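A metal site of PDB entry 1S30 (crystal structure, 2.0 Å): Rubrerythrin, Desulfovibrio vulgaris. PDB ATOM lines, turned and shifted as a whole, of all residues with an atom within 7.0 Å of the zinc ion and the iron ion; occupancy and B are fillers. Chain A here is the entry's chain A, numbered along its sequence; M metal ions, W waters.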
ATOM      1  N   GLU A  20     -25.113  15.258  27.896  1.00  0.00           N
ATOM      2  CA  GLU A  20     -25.554  16.441  28.639  1.00  0.00           C
ATOM      3  C   GLU A  20     -26.417  16.048  29.835  1.00  0.00           C
ATOM      4  O   GLU A  20     -26.322  16.651  30.907  1.00  0.00           O
ATOM      5  CB  GLU A  20     -26.331  17.388  27.722  1.00  0.00           C
ATOM      6  CG  GLU A  20     -25.477  18.015  26.622  1.00  0.00           C
ATOM      7  CD  GLU A  20     -24.496  19.050  27.147  1.00  0.00           C
ATOM      8  OE1 GLU A  20     -23.600  18.696  27.944  1.00  0.00           O
ATOM      9  OE2 GLU A  20     -24.631  20.230  26.762  1.00  0.00           O
ATOM     10  N   ALA A  23     -24.152  14.752  32.529  1.00  0.00           N
ATOM     11  CA  ALA A  23     -23.420  15.866  33.123  1.00  0.00           C
ATOM     12  C   ALA A  23     -24.299  16.609  34.123  1.00  0.00           C
ATOM     13  O   ALA A  23     -23.805  17.079  35.159  1.00  0.00           O
ATOM     14  CB  ALA A  23     -22.923  16.822  32.037  1.00  0.00           C
ATOM     15  N   TYR A  27     -23.016  17.065  37.916  1.00  0.00           N
ATOM     16  CA  TYR A  27     -22.830  18.387  38.492  1.00  0.00           C
ATOM     17  C   TYR A  27     -23.667  18.604  39.759  1.00  0.00           C
ATOM     18  O   TYR A  27     -23.208  19.216  40.722  1.00  0.00           O
ATOM     19  CB  TYR A  27     -23.116  19.490  37.452  1.00  0.00           C
ATOM     20  CG  TYR A  27     -22.148  19.517  36.289  1.00  0.00           C
ATOM     21  CD1 TYR A  27     -20.941  18.798  36.345  1.00  0.00           C
ATOM     22  CD2 TYR A  27     -22.408  20.269  35.145  1.00  0.00           C
ATOM     23  CE1 TYR A  27     -20.031  18.838  35.289  1.00  0.00           C
ATOM     24  CE2 TYR A  27     -21.491  20.315  34.087  1.00  0.00           C
ATOM     25  CZ  TYR A  27     -20.307  19.596  34.160  1.00  0.00           C
ATOM     26  OH  TYR A  27     -19.403  19.652  33.131  1.00  0.00           O
ATOM     27  N   THR A  49     -24.671  25.263  36.886  1.00  0.00           N
ATOM     28  CA  THR A  49     -24.125  24.664  35.671  1.00  0.00           C
ATOM     29  C   THR A  49     -25.023  23.487  35.292  1.00  0.00           C
ATOM     30  O   THR A  49     -25.341  23.303  34.128  1.00  0.00           O
ATOM     31  CB  THR A  49     -22.664  24.186  35.873  1.00  0.00           C
ATOM     32  OG1 THR A  49     -21.863  25.285  36.337  1.00  0.00           O
ATOM     33  CG2 THR A  49     -22.085  23.684  34.549  1.00  0.00           C
ATOM     34  N   GLN A  52     -27.972  24.607  33.614  1.00  0.00           N
ATOM     35  CA  GLN A  52     -27.688  25.057  32.258  1.00  0.00           C
ATOM     36  C   GLN A  52     -27.507  23.852  31.343  1.00  0.00           C
ATOM     37  O   GLN A  52     -27.853  23.915  30.158  1.00  0.00           O
ATOM     38  CB  GLN A  52     -26.459  25.970  32.266  1.00  0.00           C
ATOM     39  CG  GLN A  52     -26.717  27.217  33.125  1.00  0.00           C
ATOM     40  CD  GLN A  52     -25.625  28.257  33.032  1.00  0.00           C
ATOM     41  OE1 GLN A  52     -24.447  27.930  32.888  1.00  0.00           O
ATOM     42  NE2 GLN A  52     -26.021  29.517  33.138  1.00  0.00           N
ATOM     43  N   GLU A  53     -27.004  22.752  31.890  1.00  0.00           N
ATOM     44  CA  GLU A  53     -26.845  21.536  31.096  1.00  0.00           C
ATOM     45  C   GLU A  53     -28.235  21.048  30.718  1.00  0.00           C
ATOM     46  O   GLU A  53     -28.466  20.559  29.607  1.00  0.00           O
ATOM     47  CB  GLU A  53     -26.116  20.444  31.887  1.00  0.00           C
ATOM     48  CG  GLU A  53     -24.665  20.786  32.234  1.00  0.00           C
ATOM     49  CD  GLU A  53     -23.865  21.264  31.023  1.00  0.00           C
ATOM     50  OE1 GLU A  53     -24.146  20.788  29.916  1.00  0.00           O
ATOM     51  OE2 GLU A  53     -22.955  22.089  31.198  1.00  0.00           O
ATOM     52  N   ARG A  54     -29.176  21.179  31.659  1.00  0.00           N
ATOM     53  CA  ARG A  54     -30.566  20.785  31.416  1.00  0.00           C
ATOM     54  C   ARG A  54     -31.110  21.547  30.205  1.00  0.00           C
ATOM     55  O   ARG A  54     -31.840  20.983  29.377  1.00  0.00           O
ATOM     56  CB  ARG A  54     -31.427  21.109  32.636  1.00  0.00           C
ATOM     57  CG  ARG A  54     -32.935  20.925  32.420  1.00  0.00           C
ATOM     58  CD  ARG A  54     -33.720  21.573  33.555  1.00  0.00           C
ATOM     59  NE  ARG A  54     -33.528  23.028  33.569  1.00  0.00           N
ATOM     60  CZ  ARG A  54     -33.502  23.771  34.674  1.00  0.00           C
ATOM     61  NH1 ARG A  54     -33.665  23.217  35.866  1.00  0.00           N
ATOM     62  NH2 ARG A  54     -33.303  25.083  34.575  1.00  0.00           N
ATOM     63  N   GLU A  55     -30.748  22.824  30.099  1.00  0.00           N
ATOM     64  CA  GLU A  55     -31.218  23.649  29.005  1.00  0.00           C
ATOM     65  C   GLU A  55     -30.538  23.328  27.677  1.00  0.00           C
ATOM     66  O   GLU A  55     -31.163  23.403  26.628  1.00  0.00           O
ATOM     67  CB  GLU A  55     -31.045  25.133  29.364  1.00  0.00           C
ATOM     68  CG  GLU A  55     -31.891  25.571  30.554  1.00  0.00           C
ATOM     69  CD  GLU A  55     -33.376  25.305  30.357  1.00  0.00           C
ATOM     70  OE1 GLU A  55     -33.937  25.716  29.309  1.00  0.00           O
ATOM     71  OE2 GLU A  55     -33.995  24.680  31.253  1.00  0.00           O
ATOM     72  N   HIS A  56     -29.255  22.976  27.727  1.00  0.00           N
ATOM     73  CA  HIS A  56     -28.543  22.607  26.512  1.00  0.00           C
ATOM     74  C   HIS A  56     -29.224  21.344  25.976  1.00  0.00           C
ATOM     75  O   HIS A  56     -29.516  21.227  24.774  1.00  0.00           O
ATOM     76  CB  HIS A  56     -27.075  22.284  26.822  1.00  0.00           C
ATOM     77  CG  HIS A  56     -26.251  23.480  27.185  1.00  0.00           C
ATOM     78  ND1 HIS A  56     -24.969  23.374  27.674  1.00  0.00           N
ATOM     79  CD2 HIS A  56     -26.526  24.797  27.134  1.00  0.00           C
ATOM     80  CE1 HIS A  56     -24.495  24.577  27.923  1.00  0.00           C
ATOM     81  NE2 HIS A  56     -25.428  25.469  27.603  1.00  0.00           N
ATOM     82  N   ALA A  57     -29.502  20.416  26.883  1.00  0.00           N
ATOM     83  CA  ALA A  57     -30.149  19.158  26.530  1.00  0.00           C
ATOM     84  C   ALA A  57     -31.531  19.395  25.942  1.00  0.00           C
ATOM     85  O   ALA A  57     -31.903  18.755  24.965  1.00  0.00           O
ATOM     86  CB  ALA A  57     -30.255  18.254  27.772  1.00  0.00           C
ATOM     87  N   LEU A  60     -31.466  20.579  22.330  1.00  0.00           N
ATOM     88  CA  LEU A  60     -31.113  19.436  21.497  1.00  0.00           C
ATOM     89  C   LEU A  60     -32.268  18.457  21.369  1.00  0.00           C
ATOM     90  O   LEU A  60     -32.543  17.923  20.294  1.00  0.00           O
ATOM     91  CB  LEU A  60     -29.899  18.715  22.082  1.00  0.00           C
ATOM     92  CG  LEU A  60     -28.561  19.464  22.026  1.00  0.00           C
ATOM     93  CD1 LEU A  60     -27.518  18.703  22.829  1.00  0.00           C
ATOM     94  CD2 LEU A  60     -28.119  19.604  20.585  1.00  0.00           C
ATOM     95  N   SER A  90     -14.771  17.838  35.973  1.00  0.00           N
ATOM     96  CA  SER A  90     -15.822  18.561  35.265  1.00  0.00           C
ATOM     97  C   SER A  90     -15.221  19.418  34.154  1.00  0.00           C
ATOM     98  O   SER A  90     -15.745  19.463  33.040  1.00  0.00           O
ATOM     99  CB  SER A  90     -16.601  19.447  36.239  1.00  0.00           C
ATOM    100  OG  SER A  90     -17.274  18.658  37.208  1.00  0.00           O
ATOM    101  N   GLY A  93     -14.393  17.365  31.275  1.00  0.00           N
ATOM    102  CA  GLY A  93     -15.587  17.020  30.510  1.00  0.00           C
ATOM    103  C   GLY A  93     -15.997  18.177  29.621  1.00  0.00           C
ATOM    104  O   GLY A  93     -16.318  17.980  28.453  1.00  0.00           O
ATOM    105  N   GLU A  94     -15.985  19.384  30.184  1.00  0.00           N
ATOM    106  CA  GLU A  94     -16.349  20.581  29.434  1.00  0.00           C
ATOM    107  C   GLU A  94     -15.373  20.756  28.264  1.00  0.00           C
ATOM    108  O   GLU A  94     -15.778  21.034  27.134  1.00  0.00           O
ATOM    109  CB  GLU A  94     -16.283  21.822  30.331  1.00  0.00           C
ATOM    110  CG  GLU A  94     -17.313  21.870  31.459  1.00  0.00           C
ATOM    111  CD  GLU A  94     -18.751  22.066  30.974  1.00  0.00           C
ATOM    112  OE1 GLU A  94     -18.955  22.566  29.841  1.00  0.00           O
ATOM    113  OE2 GLU A  94     -19.689  21.734  31.726  1.00  0.00           O
ATOM    114  N   GLU A  97     -15.962  18.535  25.342  1.00  0.00           N
ATOM    115  CA  GLU A  97     -17.162  19.018  24.669  1.00  0.00           C
ATOM    116  C   GLU A  97     -16.982  20.205  23.719  1.00  0.00           C
ATOM    117  O   GLU A  97     -17.518  20.183  22.604  1.00  0.00           O
ATOM    118  CB  GLU A  97     -18.225  19.360  25.710  1.00  0.00           C
ATOM    119  CG  GLU A  97     -18.971  18.147  26.254  1.00  0.00           C
ATOM    120  CD  GLU A  97     -19.473  18.367  27.665  1.00  0.00           C
ATOM    121  OE1 GLU A  97     -19.827  19.510  27.990  1.00  0.00           O
ATOM    122  OE2 GLU A  97     -19.518  17.387  28.435  1.00  0.00           O
ATOM    123  N   TYR A 102     -18.644  19.027  20.213  1.00  0.00           N
ATOM    124  CA  TYR A 102     -19.453  20.009  19.519  1.00  0.00           C
ATOM    125  C   TYR A 102     -18.883  20.514  18.195  1.00  0.00           C
ATOM    126  O   TYR A 102     -19.621  20.616  17.207  1.00  0.00           O
ATOM    127  CB  TYR A 102     -19.783  21.190  20.450  1.00  0.00           C
ATOM    128  CG  TYR A 102     -20.894  20.836  21.418  1.00  0.00           C
ATOM    129  CD1 TYR A 102     -22.126  20.366  20.943  1.00  0.00           C
ATOM    130  CD2 TYR A 102     -20.718  20.958  22.794  1.00  0.00           C
ATOM    131  CE1 TYR A 102     -23.148  20.017  21.818  1.00  0.00           C
ATOM    132  CE2 TYR A 102     -21.745  20.606  23.684  1.00  0.00           C
ATOM    133  CZ  TYR A 102     -22.957  20.133  23.178  1.00  0.00           C
ATOM    134  OH  TYR A 102     -23.973  19.788  24.037  1.00  0.00           O
ATOM    135  N   ILE A 124     -23.627  26.253  21.813  1.00  0.00           N
ATOM    136  CA  ILE A 124     -23.524  25.522  23.076  1.00  0.00           C
ATOM    137  C   ILE A 124     -22.055  25.405  23.485  1.00  0.00           C
ATOM    138  O   ILE A 124     -21.705  25.570  24.655  1.00  0.00           O
ATOM    139  CB  ILE A 124     -24.137  24.114  22.957  1.00  0.00           C
ATOM    140  CG1 ILE A 124     -25.650  24.216  22.724  1.00  0.00           C
ATOM    141  CG2 ILE A 124     -23.855  23.316  24.223  1.00  0.00           C
ATOM    142  CD1 ILE A 124     -26.317  22.903  22.369  1.00  0.00           C
ATOM    143  N   ALA A 127     -20.811  28.163  25.560  1.00  0.00           N
ATOM    144  CA  ALA A 127     -21.235  28.111  26.953  1.00  0.00           C
ATOM    145  C   ALA A 127     -20.340  27.153  27.733  1.00  0.00           C
ATOM    146  O   ALA A 127     -19.946  27.438  28.854  1.00  0.00           O
ATOM    147  CB  ALA A 127     -22.689  27.658  27.055  1.00  0.00           C
ATOM    148  N   GLU A 128     -19.995  26.028  27.108  1.00  0.00           N
ATOM    149  CA  GLU A 128     -19.157  25.029  27.758  1.00  0.00           C
ATOM    150  C   GLU A 128     -17.758  25.557  28.055  1.00  0.00           C
ATOM    151  O   GLU A 128     -17.161  25.202  29.066  1.00  0.00           O
ATOM    152  CB  GLU A 128     -19.055  23.759  26.895  1.00  0.00           C
ATOM    153  CG  GLU A 128     -20.388  23.262  26.359  1.00  0.00           C
ATOM    154  CD  GLU A 128     -21.342  22.762  27.441  1.00  0.00           C
ATOM    155  OE1 GLU A 128     -21.486  23.445  28.479  1.00  0.00           O
ATOM    156  OE2 GLU A 128     -21.949  21.702  27.249  1.00  0.00           O
ATOM    157  N   GLU A 129     -17.232  26.395  27.183  1.00  0.00           N
ATOM    158  CA  GLU A 129     -15.893  26.939  27.412  1.00  0.00           C
ATOM    159  C   GLU A 129     -15.860  27.794  28.683  1.00  0.00           C
ATOM    160  O   GLU A 129     -14.902  27.736  29.446  1.00  0.00           O
ATOM    161  CB  GLU A 129     -15.398  27.744  26.201  1.00  0.00           C
ATOM    162  CG  GLU A 129     -14.067  28.443  26.439  1.00  0.00           C
ATOM    163  CD  GLU A 129     -13.283  28.695  25.156  1.00  0.00           C
ATOM    164  OE1 GLU A 129     -13.915  28.884  24.094  1.00  0.00           O
ATOM    165  OE2 GLU A 129     -12.038  28.705  25.215  1.00  0.00           O
ATOM    166  N   HIS A 131     -17.937  27.391  31.129  1.00  0.00           N
ATOM    167  CA  HIS A 131     -18.162  26.428  32.210  1.00  0.00           C
ATOM    168  C   HIS A 131     -16.805  25.905  32.659  1.00  0.00           C
ATOM    169  O   HIS A 131     -16.499  25.874  33.851  1.00  0.00           O
ATOM    170  CB  HIS A 131     -19.037  25.254  31.733  1.00  0.00           C
ATOM    171  CG  HIS A 131     -20.511  25.554  31.705  1.00  0.00           C
ATOM    172  ND1 HIS A 131     -21.425  24.690  31.168  1.00  0.00           N
ATOM    173  CD2 HIS A 131     -21.209  26.623  32.155  1.00  0.00           C
ATOM    174  CE1 HIS A 131     -22.640  25.208  31.281  1.00  0.00           C
ATOM    175  NE2 HIS A 131     -22.538  26.384  31.881  1.00  0.00           N
ATOM    176  N   GLU A 132     -15.982  25.491  31.692  1.00  0.00           N
ATOM    177  CA  GLU A 132     -14.657  24.979  32.020  1.00  0.00           C
ATOM    178  C   GLU A 132     -13.859  26.014  32.794  1.00  0.00           C
ATOM    179  O   GLU A 132     -13.236  25.691  33.803  1.00  0.00           O
ATOM    180  CB  GLU A 132     -13.872  24.605  30.761  1.00  0.00           C
ATOM    181  CG  GLU A 132     -12.510  23.996  31.116  1.00  0.00           C
ATOM    182  CD  GLU A 132     -11.496  24.065  29.998  1.00  0.00           C
ATOM    183  OE1 GLU A 132     -11.426  25.112  29.327  1.00  0.00           O
ATOM    184  OE2 GLU A 132     -10.755  23.082  29.809  1.00  0.00           O
ATOM    185  N   PHE A 135     -14.887  26.267  36.466  1.00  0.00           N
ATOM    186  CA  PHE A 135     -14.429  25.063  37.154  1.00  0.00           C
ATOM    187  C   PHE A 135     -12.936  25.086  37.403  1.00  0.00           C
ATOM    188  O   PHE A 135     -12.470  24.736  38.488  1.00  0.00           O
ATOM    189  CB  PHE A 135     -14.794  23.813  36.356  1.00  0.00           C
ATOM    190  CG  PHE A 135     -16.278  23.502  36.313  1.00  0.00           C
ATOM    191  CD1 PHE A 135     -17.081  23.737  37.426  1.00  0.00           C
ATOM    192  CD2 PHE A 135     -16.839  22.894  35.195  1.00  0.00           C
ATOM    193  CE1 PHE A 135     -18.426  23.373  37.425  1.00  0.00           C
ATOM    194  CE2 PHE A 135     -18.180  22.522  35.188  1.00  0.00           C
ATOM    195  CZ  PHE A 135     -18.983  22.758  36.301  1.00  0.00           C
HETATM  196 ZN    ZN M   1     -23.836  21.513  28.019  1.00  0.00          ZN
HETATM  197 FE    FE M   2     -21.157  22.589  30.337  1.00  0.00          FE
HETATM  198  O   HOH W   1     -21.274  20.404  29.740  1.00  0.00           O
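Four residues have an atom within 4 Å of the zinc ion: Glu 20, Glu 53, His 56 and Glu 128.
Along chain A the residues within 4 Å of the zinc ion span positions 20 to 128.
Along chain A the residues within 4 Å of the iron ion span positions 53 to 131.
The zinc ion is bound by the side-chain carboxylate of Glu 20 (2.0 Å), the side-chain carboxylate of Glu 128 (2.0 Å), the side-chain carboxylate of Glu 53 (2.1 Å) and a ring nitrogen (ND1) of His 56 (2.2 Å).
Slightly farther from the zinc ion lies the side-chain carboxylate (OE1) of Glu 20 (2.8 Å).
Water W1 lies within hydrogen-bond range of OE1 of Glu 97 and OE1 of Glu 20.
The iron ion is bound by OE2 of Glu 53 (2.1 Å), OE1 of Glu 128 (2.1 Å), OE2 of Glu 94 (2.2 Å), OE1 of Glu 94 (2.3 Å), water W1 (2.3 Å) and ND1 of His 131 (2.3 Å).
The iron ion has six donor atoms within binding distance.
The side-chain carboxylate (OE2) of Glu 94 lies close to the side-chain hydroxyl (OH) of Tyr 27, at 2.5 Å.
OH of Tyr 102 sits close to OE2 of Glu 20 (2.8 Å).
A ring nitrogen (NE2) of His 131 lies within hydrogen-bond range of the side-chain amide oxygen (OE1) of Gln 52 (2.7 Å).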
